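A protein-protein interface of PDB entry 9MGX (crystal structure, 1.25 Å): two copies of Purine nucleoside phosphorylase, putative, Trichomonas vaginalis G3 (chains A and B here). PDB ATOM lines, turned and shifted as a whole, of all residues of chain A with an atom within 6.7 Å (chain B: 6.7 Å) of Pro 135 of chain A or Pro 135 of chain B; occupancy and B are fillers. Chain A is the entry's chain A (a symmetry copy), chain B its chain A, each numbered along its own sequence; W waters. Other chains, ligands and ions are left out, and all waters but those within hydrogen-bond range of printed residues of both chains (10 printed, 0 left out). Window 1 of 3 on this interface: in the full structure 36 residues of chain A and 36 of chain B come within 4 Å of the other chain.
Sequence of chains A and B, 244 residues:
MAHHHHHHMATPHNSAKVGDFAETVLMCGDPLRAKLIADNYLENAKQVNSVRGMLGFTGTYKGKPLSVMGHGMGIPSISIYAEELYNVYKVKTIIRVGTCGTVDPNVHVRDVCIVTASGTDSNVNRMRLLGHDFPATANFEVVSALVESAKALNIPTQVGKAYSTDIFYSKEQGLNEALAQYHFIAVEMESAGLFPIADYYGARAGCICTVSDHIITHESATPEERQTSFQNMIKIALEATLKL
The backbone NH (N) of Asp 133 of chain A lies within hydrogen-bond range of the backbone carbonyl oxygen (O) of Thr 120 of chain B (2.9 Å).
N of Asp 133 of chain B is in hydrogen-bond range of O of Thr 120 of chain A, at 2.9 Å.
NZ of Lys 161 of chain B is in salt-bridge range of OD2 of Asp 199 of chain A, at 3.0 Å.
OD2 of Asp 199 of chain B lies within salt-bridge range of NZ of Lys 161 of chain A, at 3.0 Å.
The backbone NH of Ser 118 of chain B lies within hydrogen-bond range of the backbone carbonyl oxygen of Ala 136 of chain B (2.8 Å).
Of the printed residues of chain B, Asp 199 of chain A touches Lys 161 (3.0 Å).
Printed residues of chain B within 4 Å of Ser 118 of chain A: Pro 135.
The nearest printed residue of chain B that does not touch Pro 135 of chain A is Phe 184 of chain B (4.2 Å).
The nearest printed residue of chain B that does not touch Leu 129 of chain A is Gly 119 of chain B (5.5 Å).
Hydrophobic or aromatic side chains of chain A within 4 Å of the printed part of chain B: Ala 117, Leu 129, Phe 134, Pro 135, Tyr 163 and Phe 184.
Of the 20 printed residues of chain B, 13 touch a printed residue of chain A.
Among the printed residues, Asp or Glu carboxylates within 4 Å of a Lys or Arg side-chain nitrogen of the other chain: Lys 161 of chain A with Asp 199 of chain B (3.0 Å) and Asp 199 of chain A with Lys 161 of chain B (3.0 Å).
Leu 129 of chain A touches Tyr 163 of chain B, and with the chains exchanged Tyr 163 of chain A touches Leu 129 of chain B.
20 positions are printed for both chains.
Water W4 lies within hydrogen-bond range of the side-chain carboxylate of Asp 199 of chain B (2.7 Å), the backbone carbonyl oxygen of Thr 137 of chain B (2.8 Å) and the side-chain amino group of Lys 161 of chain A (3.3 Å).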
ATOM      1  N   ALA A 117     -25.691  15.711 -25.693  1.00  0.00           N
ATOM      2  CA  ALA A 117     -26.377  14.438 -25.455  1.00  0.00           C
ATOM      3  C   ALA A 117     -26.068  14.046 -24.024  1.00  0.00           C
ATOM      4  O   ALA A 117     -25.078  14.500 -23.456  1.00  0.00           O
ATOM      5  CB  ALA A 117     -25.906  13.333 -26.413  1.00  0.00           C
ATOM      6  N   SER A 118     -26.874  13.142 -23.469  1.00  0.00           N
ATOM      7  CA  SER A 118     -26.749  12.761 -22.069  1.00  0.00           C
ATOM      8  C   SER A 118     -26.855  11.258 -21.904  1.00  0.00           C
ATOM      9  O   SER A 118     -27.824  10.662 -22.370  1.00  0.00           O
ATOM     10  CB  SER A 118     -27.861  13.415 -21.257  1.00  0.00           C
ATOM     11  OG  SER A 118     -27.786  14.789 -21.492  1.00  0.00           O
ATOM     12  N   GLY A 119     -25.879  10.668 -21.222  1.00  0.00           N
ATOM     13  CA  GLY A 119     -25.975   9.285 -20.804  1.00  0.00           C
ATOM     14  C   GLY A 119     -26.809   9.170 -19.543  1.00  0.00           C
ATOM     15  O   GLY A 119     -27.263  10.165 -18.984  1.00  0.00           O
ATOM     16  N   THR A 120     -27.037   7.939 -19.097  1.00  0.00           N
ATOM     17  CA  THR A 120     -27.849   7.729 -17.905  1.00  0.00           C
ATOM     18  C   THR A 120     -27.668   6.325 -17.367  1.00  0.00           C
ATOM     19  O   THR A 120     -27.308   5.399 -18.096  1.00  0.00           O
ATOM     20  CB  THR A 120     -29.330   8.031 -18.186  1.00  0.00           C
ATOM     21  OG1 THR A 120     -30.065   8.018 -16.966  1.00  0.00           O
ATOM     22  CG2 THR A 120     -29.985   7.048 -19.139  1.00  0.00           C
ATOM     23  N   ASN A 125     -35.022   5.060 -21.187  1.00  0.00           N
ATOM     24  CA  ASN A 125     -34.831   5.137 -22.632  1.00  0.00           C
ATOM     25  C   ASN A 125     -34.732   3.761 -23.265  1.00  0.00           C
ATOM     26  O   ASN A 125     -35.235   3.556 -24.379  1.00  0.00           O
ATOM     27  CB  ASN A 125     -33.655   6.057 -22.955  1.00  0.00           C
ATOM     28  CG  ASN A 125     -33.921   7.473 -22.494  1.00  0.00           C
ATOM     29  OD1 ASN A 125     -35.084   7.881 -22.422  1.00  0.00           O
ATOM     30  ND2 ASN A 125     -32.879   8.204 -22.120  1.00  0.00           N
ATOM     31  N   LEU A 129     -37.047   2.002 -26.647  1.00  0.00           N
ATOM     32  CA  LEU A 129     -36.413   1.551 -27.881  1.00  0.00           C
ATOM     33  C   LEU A 129     -36.095   0.062 -27.823  1.00  0.00           C
ATOM     34  O   LEU A 129     -35.003  -0.388 -28.177  1.00  0.00           O
ATOM     35  CB  LEU A 129     -35.188   2.407 -28.227  1.00  0.00           C
ATOM     36  CG  LEU A 129     -34.761   2.325 -29.694  1.00  0.00           C
ATOM     37  CD1 LEU A 129     -35.841   2.837 -30.615  1.00  0.00           C
ATOM     38  CD2 LEU A 129     -33.480   3.103 -29.922  1.00  0.00           C
ATOM     39  N   ASP A 133     -29.905   0.865 -27.052  1.00  0.00           N
ATOM     40  CA  ASP A 133     -29.307   2.150 -26.689  1.00  0.00           C
ATOM     41  C   ASP A 133     -29.950   3.259 -27.510  1.00  0.00           C
ATOM     42  O   ASP A 133     -29.815   3.296 -28.742  1.00  0.00           O
ATOM     43  CB  ASP A 133     -27.801   2.200 -26.933  1.00  0.00           C
ATOM     44  CG  ASP A 133     -26.978   1.409 -25.939  1.00  0.00           C
ATOM     45  OD1 ASP A 133     -27.544   0.651 -25.156  1.00  0.00           O
ATOM     46  OD2 ASP A 133     -25.731   1.547 -25.959  1.00  0.00           O
ATOM     47  N   PHE A 134     -30.636   4.158 -26.808  1.00  0.00           N
ATOM     48  CA  PHE A 134     -31.320   5.329 -27.371  1.00  0.00           C
ATOM     49  C   PHE A 134     -30.625   6.559 -26.818  1.00  0.00           C
ATOM     50  O   PHE A 134     -30.789   6.868 -25.626  1.00  0.00           O
ATOM     51  CB  PHE A 134     -32.764   5.252 -26.877  1.00  0.00           C
ATOM     52  CG  PHE A 134     -33.692   6.369 -27.322  1.00  0.00           C
ATOM     53  CD1 PHE A 134     -33.265   7.537 -27.926  1.00  0.00           C
ATOM     54  CD2 PHE A 134     -35.042   6.222 -27.090  1.00  0.00           C
ATOM     55  CE1 PHE A 134     -34.171   8.521 -28.276  1.00  0.00           C
ATOM     56  CE2 PHE A 134     -35.934   7.210 -27.439  1.00  0.00           C
ATOM     57  CZ  PHE A 134     -35.493   8.365 -28.020  1.00  0.00           C
ATOM     58  N   PRO A 135     -29.831   7.273 -27.611  1.00  0.00           N
ATOM     59  CA  PRO A 135     -29.112   8.430 -27.071  1.00  0.00           C
ATOM     60  C   PRO A 135     -30.073   9.573 -26.816  1.00  0.00           C
ATOM     61  O   PRO A 135     -30.835   9.971 -27.701  1.00  0.00           O
ATOM     62  CB  PRO A 135     -28.124   8.786 -28.183  1.00  0.00           C
ATOM     63  CG  PRO A 135     -28.809   8.356 -29.431  1.00  0.00           C
ATOM     64  CD  PRO A 135     -29.559   7.087 -29.043  1.00  0.00           C
ATOM     65  N   ALA A 136     -30.054  10.073 -25.588  1.00  0.00           N
ATOM     66  CA  ALA A 136     -30.792  11.285 -25.258  1.00  0.00           C
ATOM     67  C   ALA A 136     -30.034  12.454 -25.863  1.00  0.00           C
ATOM     68  O   ALA A 136     -28.947  12.791 -25.393  1.00  0.00           O
ATOM     69  CB  ALA A 136     -30.903  11.398 -23.741  1.00  0.00           C
ATOM     70  N   THR A 137     -30.569  13.037 -26.931  1.00  0.00           N
ATOM     71  CA  THR A 137     -29.814  13.930 -27.802  1.00  0.00           C
ATOM     72  C   THR A 137     -30.512  15.284 -27.852  1.00  0.00           C
ATOM     73  O   THR A 137     -31.709  15.355 -28.146  1.00  0.00           O
ATOM     74  CB  THR A 137     -29.694  13.329 -29.219  1.00  0.00           C
ATOM     75  OG1 THR A 137     -29.200  11.993 -29.115  1.00  0.00           O
ATOM     76  CG2 THR A 137     -28.747  14.141 -30.093  1.00  0.00           C
ATOM     77  N   ALA A 138     -29.762  16.350 -27.592  1.00  0.00           N
ATOM     78  CA  ALA A 138     -30.302  17.693 -27.716  1.00  0.00           C
ATOM     79  C   ALA A 138     -30.552  18.040 -29.181  1.00  0.00           C
ATOM     80  O   ALA A 138     -29.866  17.564 -30.091  1.00  0.00           O
ATOM     81  CB  ALA A 138     -29.342  18.717 -27.097  1.00  0.00           C
ATOM     82  N   LYS A 161     -20.977  16.095 -23.697  1.00  0.00           N
ATOM     83  CA  LYS A 161     -21.908  15.142 -23.106  1.00  0.00           C
ATOM     84  C   LYS A 161     -22.143  15.389 -21.624  1.00  0.00           C
ATOM     85  O   LYS A 161     -21.206  15.651 -20.870  1.00  0.00           O
ATOM     86  CB  LYS A 161     -21.360  13.718 -23.243  1.00  0.00           C
ATOM     87  CG  LYS A 161     -21.220  13.205 -24.678  1.00  0.00           C
ATOM     88  CD  LYS A 161     -20.690  11.776 -24.707  1.00  0.00           C
ATOM     89  CE  LYS A 161     -19.349  11.557 -23.998  1.00  0.00           C
ATOM     90  NZ  LYS A 161     -18.265  12.301 -24.653  1.00  0.00           N
ATOM     91  N   ALA A 162     -23.388  15.189 -21.205  1.00  0.00           N
ATOM     92  CA  ALA A 162     -23.750  15.079 -19.802  1.00  0.00           C
ATOM     93  C   ALA A 162     -24.015  13.618 -19.443  1.00  0.00           C
ATOM     94  O   ALA A 162     -24.177  12.749 -20.306  1.00  0.00           O
ATOM     95  CB  ALA A 162     -24.995  15.914 -19.492  1.00  0.00           C
ATOM     96  N   TYR A 163     -24.098  13.364 -18.134  1.00  0.00           N
ATOM     97  CA  TYR A 163     -24.515  12.085 -17.573  1.00  0.00           C
ATOM     98  C   TYR A 163     -25.572  12.366 -16.526  1.00  0.00           C
ATOM     99  O   TYR A 163     -25.298  13.088 -15.564  1.00  0.00           O
ATOM    100  CB  TYR A 163     -23.346  11.357 -16.941  1.00  0.00           C
ATOM    101  CG  TYR A 163     -23.655   9.965 -16.488  1.00  0.00           C
ATOM    102  CD1 TYR A 163     -23.811   8.944 -17.407  1.00  0.00           C
ATOM    103  CD2 TYR A 163     -23.770   9.646 -15.145  1.00  0.00           C
ATOM    104  CE1 TYR A 163     -24.081   7.654 -17.015  1.00  0.00           C
ATOM    105  CE2 TYR A 163     -24.031   8.335 -14.738  1.00  0.00           C
ATOM    106  CZ  TYR A 163     -24.169   7.344 -15.686  1.00  0.00           C
ATOM    107  OH  TYR A 163     -24.394   6.041 -15.347  1.00  0.00           O
ATOM    108  N   PHE A 184     -17.100  13.066 -20.518  1.00  0.00           N
ATOM    109  CA  PHE A 184     -18.365  13.621 -20.057  1.00  0.00           C
ATOM    110  C   PHE A 184     -18.066  14.890 -19.277  1.00  0.00           C
ATOM    111  O   PHE A 184     -17.238  14.875 -18.365  1.00  0.00           O
ATOM    112  CB  PHE A 184     -19.104  12.611 -19.179  1.00  0.00           C
ATOM    113  CG  PHE A 184     -19.735  11.478 -19.955  1.00  0.00           C
ATOM    114  CD1 PHE A 184     -18.992  10.368 -20.361  1.00  0.00           C
ATOM    115  CD2 PHE A 184     -21.073  11.526 -20.301  1.00  0.00           C
ATOM    116  CE1 PHE A 184     -19.589   9.348 -21.075  1.00  0.00           C
ATOM    117  CE2 PHE A 184     -21.662  10.519 -21.011  1.00  0.00           C
ATOM    118  CZ  PHE A 184     -20.919   9.426 -21.387  1.00  0.00           C
ATOM    119  N   ALA A 192     -31.252  13.522 -19.542  1.00  0.00           N
ATOM    120  CA  ALA A 192     -31.470  12.307 -20.314  1.00  0.00           C
ATOM    121  C   ALA A 192     -32.932  11.892 -20.351  1.00  0.00           C
ATOM    122  O   ALA A 192     -33.328  11.124 -21.228  1.00  0.00           O
ATOM    123  CB  ALA A 192     -30.621  11.158 -19.774  1.00  0.00           C
ATOM    124  N   PHE A 195     -34.803  14.792 -23.318  1.00  0.00           N
ATOM    125  CA  PHE A 195     -34.602  14.786 -24.761  1.00  0.00           C
ATOM    126  C   PHE A 195     -35.476  13.756 -25.471  1.00  0.00           C
ATOM    127  O   PHE A 195     -36.030  14.084 -26.536  1.00  0.00           O
ATOM    128  CB  PHE A 195     -33.113  14.607 -25.108  1.00  0.00           C
ATOM    129  CG  PHE A 195     -32.203  15.664 -24.517  1.00  0.00           C
ATOM    130  CD1 PHE A 195     -32.645  16.967 -24.287  1.00  0.00           C
ATOM    131  CD2 PHE A 195     -30.903  15.367 -24.190  1.00  0.00           C
ATOM    132  CE1 PHE A 195     -31.796  17.930 -23.760  1.00  0.00           C
ATOM    133  CE2 PHE A 195     -30.055  16.319 -23.651  1.00  0.00           C
ATOM    134  CZ  PHE A 195     -30.497  17.610 -23.467  1.00  0.00           C
ATOM    135  N   PRO A 196     -35.657  12.532 -24.959  1.00  0.00           N
ATOM    136  CA  PRO A 196     -36.498  11.571 -25.690  1.00  0.00           C
ATOM    137  C   PRO A 196     -37.966  11.934 -25.695  1.00  0.00           C
ATOM    138  O   PRO A 196     -38.690  11.554 -26.626  1.00  0.00           O
ATOM    139  CB  PRO A 196     -36.230  10.257 -24.957  1.00  0.00           C
ATOM    140  CG  PRO A 196     -34.853  10.446 -24.399  1.00  0.00           C
ATOM    141  CD  PRO A 196     -34.898  11.853 -23.899  1.00  0.00           C
ATOM    142  N   ASP A 199     -38.422  14.259 -28.483  1.00  0.00           N
ATOM    143  CA  ASP A 199     -38.461  13.461 -29.711  1.00  0.00           C
ATOM    144  C   ASP A 199     -39.847  12.873 -29.953  1.00  0.00           C
ATOM    145  O   ASP A 199     -40.367  12.921 -31.068  1.00  0.00           O
ATOM    146  CB  ASP A 199     -37.452  12.312 -29.648  1.00  0.00           C
ATOM    147  CG  ASP A 199     -36.015  12.747 -29.727  1.00  0.00           C
ATOM    148  OD1 ASP A 199     -35.726  13.884 -30.160  1.00  0.00           O
ATOM    149  OD2 ASP A 199     -35.158  11.912 -29.351  1.00  0.00           O
ATOM    150  N   ALA B 117     -25.988  12.104 -33.044  1.00  0.00           N
ATOM    151  CA  ALA B 117     -25.740  11.009 -32.102  1.00  0.00           C
ATOM    152  C   ALA B 117     -26.352   9.766 -32.718  1.00  0.00           C
ATOM    153  O   ALA B 117     -27.239   9.865 -33.561  1.00  0.00           O
ATOM    154  CB  ALA B 117     -26.367  11.270 -30.723  1.00  0.00           C
ATOM    155  N   SER B 118     -25.928   8.596 -32.240  1.00  0.00           N
ATOM    156  CA  SER B 118     -26.358   7.332 -32.820  1.00  0.00           C
ATOM    157  C   SER B 118     -26.715   6.332 -31.738  1.00  0.00           C
ATOM    158  O   SER B 118     -25.903   6.082 -30.850  1.00  0.00           O
ATOM    159  CB  SER B 118     -25.233   6.746 -33.666  1.00  0.00           C
ATOM    160  OG  SER B 118     -24.875   7.719 -34.600  1.00  0.00           O
ATOM    161  N   GLY B 119     -27.907   5.753 -31.837  1.00  0.00           N
ATOM    162  CA  GLY B 119     -28.275   4.628 -31.006  1.00  0.00           C
ATOM    163  C   GLY B 119     -27.700   3.343 -31.569  1.00  0.00           C
ATOM    164  O   GLY B 119     -27.063   3.334 -32.619  1.00  0.00           O
ATOM    165  N   THR B 120     -27.904   2.242 -30.853  1.00  0.00           N
ATOM    166  CA  THR B 120     -27.367   0.964 -31.303  1.00  0.00           C
ATOM    167  C   THR B 120     -28.021  -0.188 -30.568  1.00  0.00           C
ATOM    168  O   THR B 120     -28.524  -0.036 -29.454  1.00  0.00           O
ATOM    169  CB  THR B 120     -25.837   0.924 -31.153  1.00  0.00           C
ATOM    170  OG1 THR B 120     -25.320  -0.244 -31.785  1.00  0.00           O
ATOM    171  CG2 THR B 120     -25.364   0.926 -29.711  1.00  0.00           C
ATOM    172  N   ASN B 125     -20.874  -0.048 -26.187  1.00  0.00           N
ATOM    173  CA  ASN B 125     -20.826   1.173 -25.389  1.00  0.00           C
ATOM    174  C   ASN B 125     -21.225   0.923 -23.946  1.00  0.00           C
ATOM    175  O   ASN B 125     -20.648   1.530 -23.032  1.00  0.00           O
ATOM    176  CB  ASN B 125     -21.627   2.277 -26.075  1.00  0.00           C
ATOM    177  CG  ASN B 125     -21.033   2.634 -27.420  1.00  0.00           C
ATOM    178  OD1 ASN B 125     -19.825   2.472 -27.614  1.00  0.00           O
ATOM    179  ND2 ASN B 125     -21.863   3.054 -28.367  1.00  0.00           N
ATOM    180  N   LEU B 129     -19.054   1.899 -20.174  1.00  0.00           N
ATOM    181  CA  LEU B 129     -19.608   2.789 -19.159  1.00  0.00           C
ATOM    182  C   LEU B 129     -20.347   2.002 -18.083  1.00  0.00           C
ATOM    183  O   LEU B 129     -21.459   2.341 -17.673  1.00  0.00           O
ATOM    184  CB  LEU B 129     -20.470   3.890 -19.788  1.00  0.00           C
ATOM    185  CG  LEU B 129     -20.688   5.107 -18.886  1.00  0.00           C
ATOM    186  CD1 LEU B 129     -19.385   5.798 -18.564  1.00  0.00           C
ATOM    187  CD2 LEU B 129     -21.643   6.089 -19.536  1.00  0.00           C
ATOM    188  N   ASP B 133     -26.085   3.638 -20.070  1.00  0.00           N
ATOM    189  CA  ASP B 133     -26.333   4.247 -21.376  1.00  0.00           C
ATOM    190  C   ASP B 133     -25.286   5.320 -21.642  1.00  0.00           C
ATOM    191  O   ASP B 133     -25.227   6.338 -20.935  1.00  0.00           O
ATOM    192  CB  ASP B 133     -27.710   4.899 -21.482  1.00  0.00           C
ATOM    193  CG  ASP B 133     -28.859   3.921 -21.594  1.00  0.00           C
ATOM    194  OD1 ASP B 133     -28.654   2.726 -21.403  1.00  0.00           O
ATOM    195  OD2 ASP B 133     -29.997   4.374 -21.869  1.00  0.00           O
ATOM    196  N   PHE B 134     -24.479   5.080 -22.673  1.00  0.00           N
ATOM    197  CA  PHE B 134     -23.413   5.976 -23.139  1.00  0.00           C
ATOM    198  C   PHE B 134     -23.795   6.434 -24.534  1.00  0.00           C
ATOM    199  O   PHE B 134     -23.722   5.634 -25.480  1.00  0.00           O
ATOM    200  CB  PHE B 134     -22.138   5.132 -23.175  1.00  0.00           C
ATOM    201  CG  PHE B 134     -20.874   5.835 -23.636  1.00  0.00           C
ATOM    202  CD1 PHE B 134     -20.855   7.081 -24.234  1.00  0.00           C
ATOM    203  CD2 PHE B 134     -19.672   5.183 -23.470  1.00  0.00           C
ATOM    204  CE1 PHE B 134     -19.663   7.642 -24.655  1.00  0.00           C
ATOM    205  CE2 PHE B 134     -18.492   5.750 -23.895  1.00  0.00           C
ATOM    206  CZ  PHE B 134     -18.494   6.975 -24.501  1.00  0.00           C
ATOM    207  N   PRO B 135     -24.227   7.679 -24.716  1.00  0.00           N
ATOM    208  CA  PRO B 135     -24.652   8.114 -26.050  1.00  0.00           C
ATOM    209  C   PRO B 135     -23.449   8.278 -26.956  1.00  0.00           C
ATOM    210  O   PRO B 135     -22.486   8.969 -26.614  1.00  0.00           O
ATOM    211  CB  PRO B 135     -25.324   9.462 -25.787  1.00  0.00           C
ATOM    212  CG  PRO B 135     -24.621   9.994 -24.589  1.00  0.00           C
ATOM    213  CD  PRO B 135     -24.332   8.765 -23.733  1.00  0.00           C
ATOM    214  N   ALA B 136     -23.499   7.609 -28.099  1.00  0.00           N
ATOM    215  CA  ALA B 136     -22.498   7.818 -29.138  1.00  0.00           C
ATOM    216  C   ALA B 136     -22.791   9.161 -29.784  1.00  0.00           C
ATOM    217  O   ALA B 136     -23.792   9.297 -30.490  1.00  0.00           O
ATOM    218  CB  ALA B 136     -22.579   6.671 -30.139  1.00  0.00           C
ATOM    219  N   THR B 137     -21.964  10.162 -29.506  1.00  0.00           N
ATOM    220  CA  THR B 137     -22.295  11.556 -29.774  1.00  0.00           C
ATOM    221  C   THR B 137     -21.237  12.152 -30.695  1.00  0.00           C
ATOM    222  O   THR B 137     -20.042  12.075 -30.399  1.00  0.00           O
ATOM    223  CB  THR B 137     -22.379  12.356 -28.456  1.00  0.00           C
ATOM    224  OG1 THR B 137     -23.246  11.670 -27.553  1.00  0.00           O
ATOM    225  CG2 THR B 137     -22.915  13.762 -28.688  1.00  0.00           C
ATOM    226  N   ALA B 138     -21.677  12.762 -31.791  1.00  0.00           N
ATOM    227  CA  ALA B 138     -20.761  13.455 -32.681  1.00  0.00           C
ATOM    228  C   ALA B 138     -20.213  14.715 -32.016  1.00  0.00           C
ATOM    229  O   ALA B 138     -20.870  15.354 -31.188  1.00  0.00           O
ATOM    230  CB  ALA B 138     -21.463  13.824 -33.994  1.00  0.00           C
ATOM    231  N   LYS B 161     -30.627  12.127 -35.242  1.00  0.00           N
ATOM    232  CA  LYS B 161     -30.105  10.867 -34.730  1.00  0.00           C
ATOM    233  C   LYS B 161     -30.025   9.785 -35.796  1.00  0.00           C
ATOM    234  O   LYS B 161     -30.944   9.616 -36.597  1.00  0.00           O
ATOM    235  CB  LYS B 161     -31.015  10.334 -33.619  1.00  0.00           C
ATOM    236  CG  LYS B 161     -31.090  11.202 -32.360  1.00  0.00           C
ATOM    237  CD  LYS B 161     -31.999  10.578 -31.309  1.00  0.00           C
ATOM    238  CE  LYS B 161     -33.433  10.291 -31.765  1.00  0.00           C
ATOM    239  NZ  LYS B 161     -34.151  11.530 -32.098  1.00  0.00           N
ATOM    240  N   ALA B 162     -28.964   8.989 -35.719  1.00  0.00           N
ATOM    241  CA  ALA B 162     -28.854   7.732 -36.441  1.00  0.00           C
ATOM    242  C   ALA B 162     -29.077   6.560 -35.487  1.00  0.00           C
ATOM    243  O   ALA B 162     -29.050   6.697 -34.260  1.00  0.00           O
ATOM    244  CB  ALA B 162     -27.479   7.599 -37.101  1.00  0.00           C
ATOM    245  N   TYR B 163     -29.259   5.376 -36.081  1.00  0.00           N
ATOM    246  CA  TYR B 163     -29.314   4.105 -35.370  1.00  0.00           C
ATOM    247  C   TYR B 163     -28.383   3.144 -36.079  1.00  0.00           C
ATOM    248  O   TYR B 163     -28.572   2.879 -37.269  1.00  0.00           O
ATOM    249  CB  TYR B 163     -30.721   3.543 -35.360  1.00  0.00           C
ATOM    250  CG  TYR B 163     -30.895   2.323 -34.512  1.00  0.00           C
ATOM    251  CD1 TYR B 163     -30.910   2.422 -33.133  1.00  0.00           C
ATOM    252  CD2 TYR B 163     -31.071   1.068 -35.071  1.00  0.00           C
ATOM    253  CE1 TYR B 163     -31.083   1.317 -32.332  1.00  0.00           C
ATOM    254  CE2 TYR B 163     -31.262  -0.057 -34.264  1.00  0.00           C
ATOM    255  CZ  TYR B 163     -31.280   0.086 -32.893  1.00  0.00           C
ATOM    256  OH  TYR B 163     -31.492  -0.972 -32.056  1.00  0.00           O
ATOM    257  N   PHE B 184     -35.628   9.081 -35.394  1.00  0.00           N
ATOM    258  CA  PHE B 184     -34.336   8.668 -35.926  1.00  0.00           C
ATOM    259  C   PHE B 184     -34.365   8.858 -37.434  1.00  0.00           C
ATOM    260  O   PHE B 184     -35.284   8.380 -38.100  1.00  0.00           O
ATOM    261  CB  PHE B 184     -34.054   7.207 -35.573  1.00  0.00           C
ATOM    262  CG  PHE B 184     -33.671   6.994 -34.127  1.00  0.00           C
ATOM    263  CD1 PHE B 184     -34.637   6.904 -33.122  1.00  0.00           C
ATOM    264  CD2 PHE B 184     -32.342   6.905 -33.759  1.00  0.00           C
ATOM    265  CE1 PHE B 184     -34.263   6.716 -31.806  1.00  0.00           C
ATOM    266  CE2 PHE B 184     -31.973   6.723 -32.457  1.00  0.00           C
ATOM    267  CZ  PHE B 184     -32.937   6.617 -31.484  1.00  0.00           C
ATOM    268  N   ALA B 192     -22.239   4.495 -34.313  1.00  0.00           N
ATOM    269  CA  ALA B 192     -22.272   4.353 -32.864  1.00  0.00           C
ATOM    270  C   ALA B 192     -21.003   3.727 -32.309  1.00  0.00           C
ATOM    271  O   ALA B 192     -20.723   3.865 -31.118  1.00  0.00           O
ATOM    272  CB  ALA B 192     -23.484   3.535 -32.425  1.00  0.00           C
ATOM    273  N   PHE B 195     -17.968   7.116 -32.475  1.00  0.00           N
ATOM    274  CA  PHE B 195     -17.953   8.292 -31.615  1.00  0.00           C
ATOM    275  C   PHE B 195     -17.321   8.015 -30.254  1.00  0.00           C
ATOM    276  O   PHE B 195     -16.549   8.866 -29.776  1.00  0.00           O
ATOM    277  CB  PHE B 195     -19.365   8.890 -31.478  1.00  0.00           C
ATOM    278  CG  PHE B 195     -20.006   9.285 -32.792  1.00  0.00           C
ATOM    279  CD1 PHE B 195     -19.245   9.708 -33.881  1.00  0.00           C
ATOM    280  CD2 PHE B 195     -21.370   9.241 -32.948  1.00  0.00           C
ATOM    281  CE1 PHE B 195     -19.847  10.082 -35.075  1.00  0.00           C
ATOM    282  CE2 PHE B 195     -21.976   9.598 -34.140  1.00  0.00           C
ATOM    283  CZ  PHE B 195     -21.211  10.050 -35.193  1.00  0.00           C
ATOM    284  N   PRO B 196     -17.576   6.881 -29.590  1.00  0.00           N
ATOM    285  CA  PRO B 196     -16.952   6.668 -28.275  1.00  0.00           C
ATOM    286  C   PRO B 196     -15.457   6.451 -28.343  1.00  0.00           C
ATOM    287  O   PRO B 196     -14.747   6.753 -27.373  1.00  0.00           O
ATOM    288  CB  PRO B 196     -17.690   5.440 -27.742  1.00  0.00           C
ATOM    289  CG  PRO B 196     -19.020   5.510 -28.429  1.00  0.00           C
ATOM    290  CD  PRO B 196     -18.642   5.896 -29.822  1.00  0.00           C
ATOM    291  N   ASP B 199     -13.954   9.788 -28.376  1.00  0.00           N
ATOM    292  CA  ASP B 199     -13.971  10.284 -26.997  1.00  0.00           C
ATOM    293  C   ASP B 199     -12.794   9.743 -26.193  1.00  0.00           C
ATOM    294  O   ASP B 199     -12.128  10.487 -25.472  1.00  0.00           O
ATOM    295  CB  ASP B 199     -15.266   9.883 -26.288  1.00  0.00           C
ATOM    296  CG  ASP B 199     -16.490  10.602 -26.784  1.00  0.00           C
ATOM    297  OD1 ASP B 199     -16.373  11.658 -27.444  1.00  0.00           O
ATOM    298  OD2 ASP B 199     -17.596  10.090 -26.489  1.00  0.00           O
HETATM  299  O   HOH W   1     -24.360   2.465 -23.697  1.00  0.00           O
HETATM  300  O   HOH W   2     -23.772  -0.445 -26.169  1.00  0.00           O
HETATM  301  O   HOH W   3     -31.356   3.526 -24.165  1.00  0.00           O
HETATM  302  O   HOH W   4     -18.792  12.695 -27.931  1.00  0.00           O
HETATM  303  O   HOH W   5     -33.067  14.145 -30.320  1.00  0.00           O
HETATM  304  O   HOH W   6     -29.231   2.601 -18.265  1.00  0.00           O
HETATM  305  O   HOH W   7     -27.485  -2.024 -26.900  1.00  0.00           O
HETATM  306  O   HOH W   8     -30.344   6.875 -22.934  1.00  0.00           O
HETATM  307  O   HOH W   9     -32.396   3.988 -20.473  1.00  0.00           O
HETATM  308  O   HOH W  10     -24.528   3.674 -27.199  1.00  0.00           O
